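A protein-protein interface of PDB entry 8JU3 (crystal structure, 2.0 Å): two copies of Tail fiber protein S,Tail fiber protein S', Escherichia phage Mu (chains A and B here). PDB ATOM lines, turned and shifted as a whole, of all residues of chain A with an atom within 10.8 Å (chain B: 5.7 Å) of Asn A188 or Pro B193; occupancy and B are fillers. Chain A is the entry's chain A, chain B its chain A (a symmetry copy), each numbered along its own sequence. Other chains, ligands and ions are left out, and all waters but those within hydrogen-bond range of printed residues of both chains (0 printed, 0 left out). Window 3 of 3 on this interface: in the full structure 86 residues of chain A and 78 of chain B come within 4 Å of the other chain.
OD1 of Asn A188 sits close to O of Pro B193.
The side-chain amide nitrogen (ND2) of Asn B201 is in hydrogen-bond range of the backbone carbonyl oxygen (O) of Asn A188, 2.7 Å away.
The side-chain hydroxyl of Thr B197 sits at hydrogen-bond distance from the side-chain amide nitrogen of Asn A188, 3.0 Å away.
O of Thr B197 lies close to OD1 of Asn B201 (3.3 Å).
O of Gly B194 sits at hydrogen-bond distance from OG1 of Thr B197, at 2.5 Å.
The side-chain amino group (NZ) of Lys A195 sits at hydrogen-bond distance from the backbone carbonyl oxygen (O) of Ala A190 (3.0 Å).
Asn A188 touches Phe B198 (C to CD2, 3.4 Å).
N of Gly A189 touches CD2 of Phe B198, at 3.4 Å.
Ala A190 touches Asn B201.
CD of Lys A195 touches O of Asn B201 (3.6 Å).
Asn A188 touches just these residues of chain B: Pro B193 (2.5 Å), Thr B197 (3.0 Å), Phe B198 (3.4 Å) and Asn B201 (2.7 Å).
Of chain A, only Asn A188 comes within 4 Å of Pro B193.
No residue of chain A comes within 4 Å of Ile B192.
No residue of chain A comes within 4 Å of Gly B194.
Printed residues of chain A within 4 Å of Phe B198: Asn A188 (3.4 Å) and Gly A189 (3.4 Å).
Of chain A, only Asn A188, Ala A190 and Lys A195 come within 4 Å of Asn B201.
Printed residues of chain B within 4 Å of Ala A190: Asn B201 (3.7 Å).
Of the printed residues of chain B, Gly A189 touches Phe B198 (3.4 Å).
Asp B191 touches none of the printed residues of chain A.
Pro A193 touches none of the printed residues of chain B.
Of the 9 printed residues of chain A, 4 touch a printed residue of chain B.
Hydrophobic or aromatic side chains of chain A that line the printed part of chain B: Ala A190.
Of the 8 printed residues of chain B, 4 touch a printed residue of chain A.
Among the printed residues, no Asp or Glu carboxylate lies within 4 Å of a Lys or Arg side-chain nitrogen of the other chain.
5 positions are printed for both chains.
Of the 7 pairs that touch across the chains among the printed residues, none has its exchanged pair printed and touching as well.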
ATOM      1  N   GLN A 187       7.012  -5.382 -20.274  1.00  0.00           N
ATOM      2  CA  GLN A 187       7.613  -4.649 -21.387  1.00  0.00           C
ATOM      3  C   GLN A 187       9.141  -4.670 -21.322  1.00  0.00           C
ATOM      4  O   GLN A 187       9.811  -5.032 -22.299  1.00  0.00           O
ATOM      5  CB  GLN A 187       7.101  -3.203 -21.433  1.00  0.00           C
ATOM      6  CG  GLN A 187       7.239  -2.339 -20.155  1.00  0.00           C
ATOM      7  CD  GLN A 187       6.213  -2.687 -19.079  1.00  0.00           C
ATOM      8  OE1 GLN A 187       5.360  -3.545 -19.290  1.00  0.00           O
ATOM      9  NE2 GLN A 187       6.233  -1.954 -17.962  1.00  0.00           N
ATOM     10  N   ASN A 188       9.693  -4.279 -20.173  1.00  0.00           N
ATOM     11  CA  ASN A 188      11.110  -4.506 -19.870  1.00  0.00           C
ATOM     12  C   ASN A 188      12.035  -3.838 -20.887  1.00  0.00           C
ATOM     13  O   ASN A 188      12.994  -4.438 -21.377  1.00  0.00           O
ATOM     14  CB  ASN A 188      11.399  -6.006 -19.779  1.00  0.00           C
ATOM     15  CG  ASN A 188      10.730  -6.648 -18.594  1.00  0.00           C
ATOM     16  OD1 ASN A 188      10.315  -5.960 -17.671  1.00  0.00           O
ATOM     17  ND2 ASN A 188      10.583  -7.967 -18.631  1.00  0.00           N
ATOM     18  N   GLY A 189      11.755  -2.575 -21.189  1.00  0.00           N
ATOM     19  CA  GLY A 189      12.561  -1.815 -22.119  1.00  0.00           C
ATOM     20  C   GLY A 189      12.577  -2.318 -23.547  1.00  0.00           C
ATOM     21  O   GLY A 189      13.222  -1.687 -24.394  1.00  0.00           O
ATOM     22  N   ALA A 190      11.903  -3.436 -23.850  1.00  0.00           N
ATOM     23  CA  ALA A 190      11.837  -3.902 -25.231  1.00  0.00           C
ATOM     24  C   ALA A 190      11.190  -2.865 -26.133  1.00  0.00           C
ATOM     25  O   ALA A 190      11.435  -2.863 -27.346  1.00  0.00           O
ATOM     26  CB  ALA A 190      11.074  -5.225 -25.306  1.00  0.00           C
ATOM     27  N   ASP A 191      10.382  -1.978 -25.556  1.00  0.00           N
ATOM     28  CA  ASP A 191       9.769  -0.867 -26.279  1.00  0.00           C
ATOM     29  C   ASP A 191      10.604   0.412 -26.131  1.00  0.00           C
ATOM     30  O   ASP A 191      10.144   1.442 -25.645  1.00  0.00           O
ATOM     31  CB  ASP A 191       8.329  -0.664 -25.800  1.00  0.00           C
ATOM     32  CG  ASP A 191       8.184  -0.775 -24.271  1.00  0.00           C
ATOM     33  OD1 ASP A 191       9.180  -1.161 -23.592  1.00  0.00           O
ATOM     34  OD2 ASP A 191       7.080  -0.440 -23.752  1.00  0.00           O
ATOM     35  N   ILE A 192      11.861   0.341 -26.568  1.00  0.00           N
ATOM     36  CA  ILE A 192      12.757   1.487 -26.554  1.00  0.00           C
ATOM     37  C   ILE A 192      13.308   1.712 -27.957  1.00  0.00           C
ATOM     38  O   ILE A 192      13.914   0.806 -28.534  1.00  0.00           O
ATOM     39  CB  ILE A 192      13.908   1.316 -25.545  1.00  0.00           C
ATOM     40  CG1 ILE A 192      13.352   1.306 -24.123  1.00  0.00           C
ATOM     41  CG2 ILE A 192      14.943   2.428 -25.693  1.00  0.00           C
ATOM     42  CD1 ILE A 192      14.404   1.183 -23.063  1.00  0.00           C
ATOM     43  N   PRO A 193      13.111   2.884 -28.559  1.00  0.00           N
ATOM     44  CA  PRO A 193      13.825   3.206 -29.797  1.00  0.00           C
ATOM     45  C   PRO A 193      15.209   3.753 -29.494  1.00  0.00           C
ATOM     46  O   PRO A 193      15.439   4.383 -28.460  1.00  0.00           O
ATOM     47  CB  PRO A 193      12.935   4.268 -30.448  1.00  0.00           C
ATOM     48  CG  PRO A 193      12.288   4.967 -29.287  1.00  0.00           C
ATOM     49  CD  PRO A 193      12.180   3.955 -28.158  1.00  0.00           C
ATOM     50  N   LYS A 195      18.051   2.154 -28.532  1.00  0.00           N
ATOM     51  CA  LYS A 195      18.484   1.679 -27.215  1.00  0.00           C
ATOM     52  C   LYS A 195      19.954   2.009 -26.914  1.00  0.00           C
ATOM     53  O   LYS A 195      20.327   2.202 -25.745  1.00  0.00           O
ATOM     54  CB  LYS A 195      18.234   0.170 -27.131  1.00  0.00           C
ATOM     55  CG  LYS A 195      16.777  -0.199 -27.388  1.00  0.00           C
ATOM     56  CD  LYS A 195      16.461  -1.698 -27.299  1.00  0.00           C
ATOM     57  CE  LYS A 195      14.932  -1.902 -27.521  1.00  0.00           C
ATOM     58  NZ  LYS A 195      14.429  -3.311 -27.454  1.00  0.00           N
ATOM     59  N   PHE A 198      19.981   5.433 -25.506  1.00  0.00           N
ATOM     60  CA  PHE A 198      19.488   5.292 -24.138  1.00  0.00           C
ATOM     61  C   PHE A 198      20.623   4.953 -23.178  1.00  0.00           C
ATOM     62  O   PHE A 198      20.859   5.642 -22.177  1.00  0.00           O
ATOM     63  CB  PHE A 198      18.425   4.187 -24.102  1.00  0.00           C
ATOM     64  CG  PHE A 198      17.692   4.077 -22.790  1.00  0.00           C
ATOM     65  CD1 PHE A 198      18.247   3.380 -21.718  1.00  0.00           C
ATOM     66  CD2 PHE A 198      16.426   4.643 -22.641  1.00  0.00           C
ATOM     67  CE1 PHE A 198      17.572   3.272 -20.512  1.00  0.00           C
ATOM     68  CE2 PHE A 198      15.737   4.539 -21.442  1.00  0.00           C
ATOM     69  CZ  PHE A 198      16.308   3.849 -20.375  1.00  0.00           C
ATOM     70  N   ASP B 191      10.483   0.930 -10.353  1.00  0.00           N
ATOM     71  CA  ASP B 191       9.254   0.286 -10.811  1.00  0.00           C
ATOM     72  C   ASP B 191       9.484  -0.457 -12.133  1.00  0.00           C
ATOM     73  O   ASP B 191       8.850  -0.196 -13.152  1.00  0.00           O
ATOM     74  CB  ASP B 191       8.135   1.324 -10.931  1.00  0.00           C
ATOM     75  CG  ASP B 191       8.606   2.646 -11.566  1.00  0.00           C
ATOM     76  OD1 ASP B 191       9.843   2.811 -11.776  1.00  0.00           O
ATOM     77  OD2 ASP B 191       7.729   3.499 -11.884  1.00  0.00           O
ATOM     78  N   ILE B 192      10.412  -1.416 -12.110  1.00  0.00           N
ATOM     79  CA  ILE B 192      10.699  -2.252 -13.266  1.00  0.00           C
ATOM     80  C   ILE B 192      10.567  -3.717 -12.871  1.00  0.00           C
ATOM     81  O   ILE B 192      11.239  -4.169 -11.940  1.00  0.00           O
ATOM     82  CB  ILE B 192      12.097  -1.976 -13.851  1.00  0.00           C
ATOM     83  CG1 ILE B 192      12.143  -0.565 -14.436  1.00  0.00           C
ATOM     84  CG2 ILE B 192      12.456  -2.998 -14.926  1.00  0.00           C
ATOM     85  CD1 ILE B 192      13.456  -0.217 -15.069  1.00  0.00           C
ATOM     86  N   PRO B 193       9.706  -4.496 -13.524  1.00  0.00           N
ATOM     87  CA  PRO B 193       9.730  -5.948 -13.327  1.00  0.00           C
ATOM     88  C   PRO B 193      10.776  -6.595 -14.217  1.00  0.00           C
ATOM     89  O   PRO B 193      11.080  -6.111 -15.307  1.00  0.00           O
ATOM     90  CB  PRO B 193       8.314  -6.379 -13.722  1.00  0.00           C
ATOM     91  CG  PRO B 193       7.902  -5.373 -14.758  1.00  0.00           C
ATOM     92  CD  PRO B 193       8.630  -4.077 -14.441  1.00  0.00           C
ATOM     93  N   GLY B 194      11.345  -7.694 -13.722  1.00  0.00           N
ATOM     94  CA  GLY B 194      12.435  -8.377 -14.403  1.00  0.00           C
ATOM     95  C   GLY B 194      13.598  -7.498 -14.844  1.00  0.00           C
ATOM     96  O   GLY B 194      13.994  -7.528 -16.014  1.00  0.00           O
ATOM     97  N   LYS B 195      14.159  -6.723 -13.913  1.00  0.00           N
ATOM     98  CA  LYS B 195      15.189  -5.735 -14.251  1.00  0.00           C
ATOM     99  C   LYS B 195      16.395  -6.354 -14.974  1.00  0.00           C
ATOM    100  O   LYS B 195      17.047  -5.684 -15.791  1.00  0.00           O
ATOM    101  CB  LYS B 195      15.627  -5.024 -12.966  1.00  0.00           C
ATOM    102  CG  LYS B 195      14.464  -4.364 -12.235  1.00  0.00           C
ATOM    103  CD  LYS B 195      14.844  -3.619 -10.948  1.00  0.00           C
ATOM    104  CE  LYS B 195      13.565  -2.952 -10.359  1.00  0.00           C
ATOM    105  NZ  LYS B 195      13.744  -2.160  -9.100  1.00  0.00           N
ATOM    106  N   THR B 197      16.266  -8.763 -17.212  1.00  0.00           N
ATOM    107  CA  THR B 197      15.868  -8.851 -18.610  1.00  0.00           C
ATOM    108  C   THR B 197      15.950  -7.482 -19.282  1.00  0.00           C
ATOM    109  O   THR B 197      16.367  -7.376 -20.444  1.00  0.00           O
ATOM    110  CB  THR B 197      14.446  -9.400 -18.698  1.00  0.00           C
ATOM    111  OG1 THR B 197      13.555  -8.369 -18.284  1.00  0.00           O
ATOM    112  CG2 THR B 197      14.262 -10.601 -17.738  1.00  0.00           C
ATOM    113  N   PHE B 198      15.520  -6.431 -18.571  1.00  0.00           N
ATOM    114  CA  PHE B 198      15.654  -5.049 -19.030  1.00  0.00           C
ATOM    115  C   PHE B 198      17.089  -4.747 -19.447  1.00  0.00           C
ATOM    116  O   PHE B 198      17.363  -4.312 -20.573  1.00  0.00           O
ATOM    117  CB  PHE B 198      15.228  -4.105 -17.900  1.00  0.00           C
ATOM    118  CG  PHE B 198      15.128  -2.657 -18.310  1.00  0.00           C
ATOM    119  CD1 PHE B 198      16.262  -1.851 -18.363  1.00  0.00           C
ATOM    120  CD2 PHE B 198      13.887  -2.094 -18.607  1.00  0.00           C
ATOM    121  CE1 PHE B 198      16.173  -0.518 -18.733  1.00  0.00           C
ATOM    122  CE2 PHE B 198      13.781  -0.761 -18.975  1.00  0.00           C
ATOM    123  CZ  PHE B 198      14.925   0.032 -19.035  1.00  0.00           C
ATOM    124  N   ASN B 201      17.974  -6.481 -22.689  1.00  0.00           N
ATOM    125  CA  ASN B 201      17.356  -5.815 -23.838  1.00  0.00           C
ATOM    126  C   ASN B 201      18.079  -4.527 -24.205  1.00  0.00           C
ATOM    127  O   ASN B 201      18.256  -4.222 -25.391  1.00  0.00           O
ATOM    128  CB  ASN B 201      15.881  -5.491 -23.561  1.00  0.00           C
ATOM    129  CG  ASN B 201      15.010  -6.725 -23.387  1.00  0.00           C
ATOM    130  OD1 ASN B 201      15.443  -7.861 -23.587  1.00  0.00           O
ATOM    131  ND2 ASN B 201      13.764  -6.497 -23.021  1.00  0.00           N
